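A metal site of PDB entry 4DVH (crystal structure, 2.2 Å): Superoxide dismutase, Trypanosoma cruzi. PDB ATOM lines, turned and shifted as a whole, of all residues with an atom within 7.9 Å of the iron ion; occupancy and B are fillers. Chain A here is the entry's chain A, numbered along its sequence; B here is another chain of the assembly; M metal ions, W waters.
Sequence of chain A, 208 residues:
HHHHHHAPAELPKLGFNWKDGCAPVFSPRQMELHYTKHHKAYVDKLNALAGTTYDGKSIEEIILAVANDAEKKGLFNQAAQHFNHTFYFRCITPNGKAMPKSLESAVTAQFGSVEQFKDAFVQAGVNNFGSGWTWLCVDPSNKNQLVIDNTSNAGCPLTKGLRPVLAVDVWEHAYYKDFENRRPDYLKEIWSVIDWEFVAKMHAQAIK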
ATOM      1  N   LEU A  33     -17.224   8.864  11.888  1.00  0.00           N
ATOM      2  CA  LEU A  33     -17.932   9.164  10.647  1.00  0.00           C
ATOM      3  C   LEU A  33     -19.270   9.833  10.941  1.00  0.00           C
ATOM      4  O   LEU A  33     -19.579  10.876  10.378  1.00  0.00           O
ATOM      5  CB  LEU A  33     -18.179   7.883   9.847  1.00  0.00           C
ATOM      6  CG  LEU A  33     -16.944   7.176   9.288  1.00  0.00           C
ATOM      7  CD1 LEU A  33     -17.286   5.728   8.909  1.00  0.00           C
ATOM      8  CD2 LEU A  33     -16.325   7.965   8.108  1.00  0.00           C
ATOM      9  N   HIS A  34     -20.056   9.251  11.853  1.00  0.00           N
ATOM     10  CA  HIS A  34     -21.378   9.783  12.156  1.00  0.00           C
ATOM     11  C   HIS A  34     -21.405  11.236  12.637  1.00  0.00           C
ATOM     12  O   HIS A  34     -22.195  12.043  12.136  1.00  0.00           O
ATOM     13  CB  HIS A  34     -22.150   8.850  13.080  1.00  0.00           C
ATOM     14  CG  HIS A  34     -23.630   8.952  12.911  1.00  0.00           C
ATOM     15  ND1 HIS A  34     -24.489   8.219  13.695  1.00  0.00           N
ATOM     16  CD2 HIS A  34     -24.356   9.697  12.050  1.00  0.00           C
ATOM     17  CE1 HIS A  34     -25.703   8.542  13.295  1.00  0.00           C
ATOM     18  NE2 HIS A  34     -25.670   9.439  12.307  1.00  0.00           N
ATOM     19  N   TYR A  35     -20.549  11.553  13.583  1.00  0.00           N
ATOM     20  CA  TYR A  35     -20.479  12.880  14.188  1.00  0.00           C
ATOM     21  C   TYR A  35     -19.637  13.872  13.384  1.00  0.00           C
ATOM     22  O   TYR A  35     -20.114  14.959  13.045  1.00  0.00           O
ATOM     23  CB  TYR A  35     -19.931  12.699  15.623  1.00  0.00           C
ATOM     24  CG  TYR A  35     -19.735  13.950  16.439  1.00  0.00           C
ATOM     25  CD1 TYR A  35     -20.834  14.698  16.869  1.00  0.00           C
ATOM     26  CD2 TYR A  35     -18.484  14.292  16.935  1.00  0.00           C
ATOM     27  CE1 TYR A  35     -20.655  15.842  17.656  1.00  0.00           C
ATOM     28  CE2 TYR A  35     -18.303  15.405  17.740  1.00  0.00           C
ATOM     29  CZ  TYR A  35     -19.382  16.194  18.073  1.00  0.00           C
ATOM     30  OH  TYR A  35     -19.119  17.244  18.902  1.00  0.00           O
ATOM     31  N   HIS A  38     -20.994  13.154   8.913  1.00  0.00           N
ATOM     32  CA  HIS A  38     -22.420  13.340   8.704  1.00  0.00           C
ATOM     33  C   HIS A  38     -22.991  14.514   9.505  1.00  0.00           C
ATOM     34  O   HIS A  38     -23.501  15.443   8.899  1.00  0.00           O
ATOM     35  CB  HIS A  38     -23.216  12.030   8.936  1.00  0.00           C
ATOM     36  CG  HIS A  38     -22.817  10.926   8.006  1.00  0.00           C
ATOM     37  ND1 HIS A  38     -23.323  10.869   6.725  1.00  0.00           N
ATOM     38  CD2 HIS A  38     -21.946   9.918   8.184  1.00  0.00           C
ATOM     39  CE1 HIS A  38     -22.759   9.812   6.162  1.00  0.00           C
ATOM     40  NE2 HIS A  38     -21.929   9.201   7.011  1.00  0.00           N
ATOM     41  N   HIS A  39     -22.889  14.530  10.843  1.00  0.00           N
ATOM     42  CA  HIS A  39     -23.470  15.638  11.611  1.00  0.00           C
ATOM     43  C   HIS A  39     -22.801  16.975  11.270  1.00  0.00           C
ATOM     44  O   HIS A  39     -23.504  17.966  11.062  1.00  0.00           O
ATOM     45  CB  HIS A  39     -23.459  15.336  13.129  1.00  0.00           C
ATOM     46  CG  HIS A  39     -24.323  16.230  13.980  1.00  0.00           C
ATOM     47  ND1 HIS A  39     -24.445  16.019  15.339  1.00  0.00           N
ATOM     48  CD2 HIS A  39     -25.078  17.306  13.642  1.00  0.00           C
ATOM     49  CE1 HIS A  39     -25.239  16.988  15.778  1.00  0.00           C
ATOM     50  NE2 HIS A  39     -25.629  17.788  14.788  1.00  0.00           N
ATOM     51  N   TYR A  42     -24.150  18.506   8.178  1.00  0.00           N
ATOM     52  CA  TYR A  42     -25.474  19.078   8.413  1.00  0.00           C
ATOM     53  C   TYR A  42     -25.347  20.468   9.032  1.00  0.00           C
ATOM     54  O   TYR A  42     -26.012  21.409   8.575  1.00  0.00           O
ATOM     55  CB  TYR A  42     -26.350  18.134   9.252  1.00  0.00           C
ATOM     56  CG  TYR A  42     -26.786  16.867   8.540  1.00  0.00           C
ATOM     57  CD1 TYR A  42     -27.491  16.919   7.334  1.00  0.00           C
ATOM     58  CD2 TYR A  42     -26.524  15.620   9.089  1.00  0.00           C
ATOM     59  CE1 TYR A  42     -27.922  15.751   6.694  1.00  0.00           C
ATOM     60  CE2 TYR A  42     -26.917  14.437   8.431  1.00  0.00           C
ATOM     61  CZ  TYR A  42     -27.638  14.513   7.250  1.00  0.00           C
ATOM     62  OH  TYR A  42     -28.061  13.346   6.659  1.00  0.00           O
ATOM     63  N   GLN A  81     -32.110  17.696  10.412  1.00  0.00           N
ATOM     64  CA  GLN A  81     -31.067  16.707  10.635  1.00  0.00           C
ATOM     65  C   GLN A  81     -30.111  17.123  11.752  1.00  0.00           C
ATOM     66  O   GLN A  81     -29.636  16.270  12.474  1.00  0.00           O
ATOM     67  CB  GLN A  81     -30.314  16.359   9.348  1.00  0.00           C
ATOM     68  CG  GLN A  81     -31.112  15.472   8.384  1.00  0.00           C
ATOM     69  CD  GLN A  81     -31.358  14.070   8.877  1.00  0.00           C
ATOM     70  OE1 GLN A  81     -32.284  13.831   9.623  1.00  0.00           O
ATOM     71  NE2 GLN A  81     -30.537  13.095   8.464  1.00  0.00           N
ATOM     72  N   ASN A  84     -32.156  16.418  14.921  1.00  0.00           N
ATOM     73  CA  ASN A  84     -32.247  14.941  15.025  1.00  0.00           C
ATOM     74  C   ASN A  84     -30.953  14.302  15.492  1.00  0.00           C
ATOM     75  O   ASN A  84     -31.011  13.427  16.355  1.00  0.00           O
ATOM     76  CB  ASN A  84     -32.704  14.322  13.700  1.00  0.00           C
ATOM     77  CG  ASN A  84     -34.108  14.691  13.284  1.00  0.00           C
ATOM     78  OD1 ASN A  84     -34.863  15.301  14.030  1.00  0.00           O
ATOM     79  ND2 ASN A  84     -34.459  14.393  12.034  1.00  0.00           N
ATOM     80  N   HIS A  85     -29.792  14.727  14.941  1.00  0.00           N
ATOM     81  CA  HIS A  85     -28.504  14.150  15.357  1.00  0.00           C
ATOM     82  C   HIS A  85     -28.117  14.603  16.745  1.00  0.00           C
ATOM     83  O   HIS A  85     -27.548  13.818  17.508  1.00  0.00           O
ATOM     84  CB  HIS A  85     -27.399  14.441  14.344  1.00  0.00           C
ATOM     85  CG  HIS A  85     -27.504  13.597  13.107  1.00  0.00           C
ATOM     86  ND1 HIS A  85     -28.231  14.016  12.013  1.00  0.00           N
ATOM     87  CD2 HIS A  85     -27.014  12.356  12.848  1.00  0.00           C
ATOM     88  CE1 HIS A  85     -28.172  13.022  11.134  1.00  0.00           C
ATOM     89  NE2 HIS A  85     -27.448  12.009  11.594  1.00  0.00           N
ATOM     90  N   TYR A  88     -30.249  12.410  19.076  1.00  0.00           N
ATOM     91  CA  TYR A  88     -29.729  11.027  19.031  1.00  0.00           C
ATOM     92  C   TYR A  88     -28.406  10.859  19.770  1.00  0.00           C
ATOM     93  O   TYR A  88     -28.254   9.904  20.546  1.00  0.00           O
ATOM     94  CB  TYR A  88     -29.589  10.591  17.580  1.00  0.00           C
ATOM     95  CG  TYR A  88     -28.869   9.269  17.360  1.00  0.00           C
ATOM     96  CD1 TYR A  88     -29.516   8.064  17.610  1.00  0.00           C
ATOM     97  CD2 TYR A  88     -27.612   9.232  16.763  1.00  0.00           C
ATOM     98  CE1 TYR A  88     -28.884   6.849  17.342  1.00  0.00           C
ATOM     99  CE2 TYR A  88     -26.976   8.023  16.488  1.00  0.00           C
ATOM    100  CZ  TYR A  88     -27.619   6.833  16.767  1.00  0.00           C
ATOM    101  OH  TYR A  88     -27.022   5.649  16.448  1.00  0.00           O
ATOM    102  N   PHE A  89     -27.445  11.777  19.548  1.00  0.00           N
ATOM    103  CA  PHE A  89     -26.137  11.708  20.233  1.00  0.00           C
ATOM    104  C   PHE A  89     -26.238  11.921  21.733  1.00  0.00           C
ATOM    105  O   PHE A  89     -25.389  11.417  22.454  1.00  0.00           O
ATOM    106  CB  PHE A  89     -25.109  12.639  19.587  1.00  0.00           C
ATOM    107  CG  PHE A  89     -24.596  12.164  18.252  1.00  0.00           C
ATOM    108  CD1 PHE A  89     -24.162  10.859  18.078  1.00  0.00           C
ATOM    109  CD2 PHE A  89     -24.521  13.035  17.166  1.00  0.00           C
ATOM    110  CE1 PHE A  89     -23.681  10.421  16.841  1.00  0.00           C
ATOM    111  CE2 PHE A  89     -24.034  12.602  15.936  1.00  0.00           C
ATOM    112  CZ  PHE A  89     -23.624  11.298  15.778  1.00  0.00           C
ATOM    113  N   GLY A 132     -34.303   7.054   7.692  1.00  0.00           N
ATOM    114  CA  GLY A 132     -35.260   7.595   8.649  1.00  0.00           C
ATOM    115  C   GLY A 132     -34.844   7.596  10.103  1.00  0.00           C
ATOM    116  O   GLY A 132     -33.668   7.421  10.462  1.00  0.00           O
ATOM    117  N   TRP A 133     -35.846   7.801  10.950  1.00  0.00           N
ATOM    118  CA  TRP A 133     -35.702   7.892  12.392  1.00  0.00           C
ATOM    119  C   TRP A 133     -36.878   7.206  13.028  1.00  0.00           C
ATOM    120  O   TRP A 133     -37.986   7.275  12.505  1.00  0.00           O
ATOM    121  CB  TRP A 133     -35.720   9.365  12.823  1.00  0.00           C
ATOM    122  CG  TRP A 133     -34.604  10.188  12.225  1.00  0.00           C
ATOM    123  CD1 TRP A 133     -34.590  10.813  11.023  1.00  0.00           C
ATOM    124  CD2 TRP A 133     -33.335  10.456  12.827  1.00  0.00           C
ATOM    125  NE1 TRP A 133     -33.389  11.435  10.821  1.00  0.00           N
ATOM    126  CE2 TRP A 133     -32.582  11.200  11.903  1.00  0.00           C
ATOM    127  CE3 TRP A 133     -32.757  10.130  14.070  1.00  0.00           C
ATOM    128  CZ2 TRP A 133     -31.275  11.645  12.175  1.00  0.00           C
ATOM    129  CZ3 TRP A 133     -31.467  10.600  14.353  1.00  0.00           C
ATOM    130  CH2 TRP A 133     -30.731  11.329  13.407  1.00  0.00           C
ATOM    131  N   ASP A 169     -31.560   6.787  15.078  1.00  0.00           N
ATOM    132  CA  ASP A 169     -31.256   6.988  13.660  1.00  0.00           C
ATOM    133  C   ASP A 169     -31.261   5.634  12.927  1.00  0.00           C
ATOM    134  O   ASP A 169     -30.596   4.682  13.362  1.00  0.00           O
ATOM    135  CB  ASP A 169     -29.861   7.635  13.523  1.00  0.00           C
ATOM    136  CG  ASP A 169     -29.537   8.271  12.183  1.00  0.00           C
ATOM    137  OD1 ASP A 169     -30.327   8.093  11.221  1.00  0.00           O
ATOM    138  OD2 ASP A 169     -28.537   8.993  12.105  1.00  0.00           O
ATOM    139  N   VAL A 170     -32.046   5.547  11.830  1.00  0.00           N
ATOM    140  CA  VAL A 170     -32.099   4.341  10.993  1.00  0.00           C
ATOM    141  C   VAL A 170     -31.580   4.588   9.568  1.00  0.00           C
ATOM    142  O   VAL A 170     -31.741   3.722   8.697  1.00  0.00           O
ATOM    143  CB  VAL A 170     -33.377   3.449  11.107  1.00  0.00           C
ATOM    144  CG1 VAL A 170     -33.571   2.961  12.534  1.00  0.00           C
ATOM    145  CG2 VAL A 170     -34.638   4.162  10.608  1.00  0.00           C
ATOM    146  N   TRP A 171     -30.938   5.769   9.338  1.00  0.00           N
ATOM    147  CA  TRP A 171     -30.231   6.047   8.079  1.00  0.00           C
ATOM    148  C   TRP A 171     -29.105   5.015   8.142  1.00  0.00           C
ATOM    149  O   TRP A 171     -28.602   4.736   9.238  1.00  0.00           O
ATOM    150  CB  TRP A 171     -29.609   7.451   8.097  1.00  0.00           C
ATOM    151  CG  TRP A 171     -30.515   8.567   7.688  1.00  0.00           C
ATOM    152  CD1 TRP A 171     -31.614   9.029   8.351  1.00  0.00           C
ATOM    153  CD2 TRP A 171     -30.296   9.481   6.594  1.00  0.00           C
ATOM    154  NE1 TRP A 171     -32.133  10.137   7.718  1.00  0.00           N
ATOM    155  CE2 TRP A 171     -31.328  10.448   6.646  1.00  0.00           C
ATOM    156  CE3 TRP A 171     -29.338   9.563   5.562  1.00  0.00           C
ATOM    157  CZ2 TRP A 171     -31.436  11.471   5.681  1.00  0.00           C
ATOM    158  CZ3 TRP A 171     -29.444  10.583   4.624  1.00  0.00           C
ATOM    159  CH2 TRP A 171     -30.477  11.532   4.689  1.00  0.00           C
ATOM    160  N   GLU A 172     -28.763   4.386   7.007  1.00  0.00           N
ATOM    161  CA  GLU A 172     -27.761   3.304   6.983  1.00  0.00           C
ATOM    162  C   GLU A 172     -26.403   3.664   7.543  1.00  0.00           C
ATOM    163  O   GLU A 172     -25.759   2.824   8.160  1.00  0.00           O
ATOM    164  CB  GLU A 172     -27.669   2.665   5.590  1.00  0.00           C
ATOM    165  CG  GLU A 172     -28.997   2.117   5.076  1.00  0.00           C
ATOM    166  CD  GLU A 172     -28.886   1.498   3.698  1.00  0.00           C
ATOM    167  OE1 GLU A 172     -28.334   2.163   2.790  1.00  0.00           O
ATOM    168  OE2 GLU A 172     -29.273   0.323   3.552  1.00  0.00           O
ATOM    169  N   HIS A 173     -25.980   4.925   7.352  1.00  0.00           N
ATOM    170  CA  HIS A 173     -24.703   5.442   7.882  1.00  0.00           C
ATOM    171  C   HIS A 173     -24.607   5.357   9.405  1.00  0.00           C
ATOM    172  O   HIS A 173     -23.486   5.380   9.927  1.00  0.00           O
ATOM    173  CB  HIS A 173     -24.442   6.915   7.430  1.00  0.00           C
ATOM    174  CG  HIS A 173     -25.368   7.961   7.971  1.00  0.00           C
ATOM    175  ND1 HIS A 173     -26.036   8.845   7.132  1.00  0.00           N
ATOM    176  CD2 HIS A 173     -25.640   8.309   9.254  1.00  0.00           C
ATOM    177  CE1 HIS A 173     -26.715   9.671   7.919  1.00  0.00           C
ATOM    178  NE2 HIS A 173     -26.513   9.383   9.203  1.00  0.00           N
ATOM    179  N   ALA A 174     -25.774   5.275  10.127  1.00  0.00           N
ATOM    180  CA  ALA A 174     -25.785   5.201  11.595  1.00  0.00           C
ATOM    181  C   ALA A 174     -25.223   3.887  12.122  1.00  0.00           C
ATOM    182  O   ALA A 174     -24.738   3.841  13.260  1.00  0.00           O
ATOM    183  CB  ALA A 174     -27.187   5.404  12.133  1.00  0.00           C
ATOM    184  N   TYR A 175     -25.311   2.804  11.312  1.00  0.00           N
ATOM    185  CA  TYR A 175     -24.902   1.486  11.744  1.00  0.00           C
ATOM    186  C   TYR A 175     -24.018   0.698  10.765  1.00  0.00           C
ATOM    187  O   TYR A 175     -23.542  -0.368  11.148  1.00  0.00           O
ATOM    188  CB  TYR A 175     -26.149   0.648  12.095  1.00  0.00           C
ATOM    189  CG  TYR A 175     -27.146   0.495  10.961  1.00  0.00           C
ATOM    190  CD1 TYR A 175     -27.024  -0.526  10.024  1.00  0.00           C
ATOM    191  CD2 TYR A 175     -28.250   1.330  10.858  1.00  0.00           C
ATOM    192  CE1 TYR A 175     -27.945  -0.671   8.984  1.00  0.00           C
ATOM    193  CE2 TYR A 175     -29.178   1.190   9.833  1.00  0.00           C
ATOM    194  CZ  TYR A 175     -29.021   0.195   8.896  1.00  0.00           C
ATOM    195  OH  TYR A 175     -29.946   0.053   7.899  1.00  0.00           O
ATOM    196  N   TYR A 186     -28.559  -3.930  15.103  1.00  0.00           N
ATOM    197  CA  TYR A 186     -28.271  -2.577  15.585  1.00  0.00           C
ATOM    198  C   TYR A 186     -29.357  -2.120  16.538  1.00  0.00           C
ATOM    199  O   TYR A 186     -29.049  -1.613  17.624  1.00  0.00           O
ATOM    200  CB  TYR A 186     -28.141  -1.620  14.374  1.00  0.00           C
ATOM    201  CG  TYR A 186     -28.378  -0.141  14.653  1.00  0.00           C
ATOM    202  CD1 TYR A 186     -27.458   0.604  15.395  1.00  0.00           C
ATOM    203  CD2 TYR A 186     -29.479   0.517  14.115  1.00  0.00           C
ATOM    204  CE1 TYR A 186     -27.613   1.984  15.553  1.00  0.00           C
ATOM    205  CE2 TYR A 186     -29.669   1.881  14.310  1.00  0.00           C
ATOM    206  CZ  TYR A 186     -28.724   2.613  15.028  1.00  0.00           C
ATOM    207  OH  TYR A 186     -28.891   3.956  15.233  1.00  0.00           O
ATOM    208  N   GLU B 172     -27.097   4.518   0.859  1.00  0.00           N
ATOM    209  CA  GLU B 172     -25.772   4.492   1.503  1.00  0.00           C
ATOM    210  C   GLU B 172     -25.084   3.130   1.474  1.00  0.00           C
ATOM    211  O   GLU B 172     -23.863   3.072   1.369  1.00  0.00           O
ATOM    212  CB  GLU B 172     -25.835   5.096   2.926  1.00  0.00           C
ATOM    213  CG  GLU B 172     -26.355   6.527   2.954  1.00  0.00           C
ATOM    214  CD  GLU B 172     -26.389   7.143   4.333  1.00  0.00           C
ATOM    215  OE1 GLU B 172     -26.965   6.537   5.262  1.00  0.00           O
ATOM    216  OE2 GLU B 172     -25.817   8.250   4.501  1.00  0.00           O
HETATM  217 FE    FE M   1     -27.267  10.044  11.043  1.00  0.00          FE
HETATM  218  O   HOH W   1     -29.193  10.459   9.769  1.00  0.00           O
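The side-chain carboxylate (OD1) of Asp 169 is in hydrogen-bond range of the backbone NH (N) of Trp 171 (3.1 Å).
O of Asp 169 lies within hydrogen-bond range of OH of Tyr 186.
A ring nitrogen (ND1) of His 85 lies within hydrogen-bond range of the backbone carbonyl oxygen (O) of Gln 81, at 2.7 Å.
A ring nitrogen (ND1) of His 173 lies within hydrogen-bond range of a ring nitrogen (ND1) of His 38 (3.4 Å).
The side-chain carboxylate (OE2) of Glu 172 of chain B is in hydrogen-bond range of a ring nitrogen (ND1) of His 173 (2.7 Å).
O of His 34 sits at hydrogen-bond distance from N of His 39 (2.9 Å).
Within 4 Å of the iron ion: His 34, His 85, Asp 169 and His 173.
The nearest printed residue that does not touch the iron ion is Trp 133 (4.4 Å).
The iron ion is bound by the side-chain carboxylate (OD2) of Asp 169, a ring nitrogen (NE2) of His 85, a ring nitrogen (NE2) of His 173, a ring nitrogen (NE2) of His 34 and water W1.
The iron ion has five donor atoms within binding distance.
Water W1 lies within hydrogen-bond range of the side-chain carboxylate of Asp 169 (3.0 Å) and the side-chain amide nitrogen of Gln 81 (3.2 Å).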
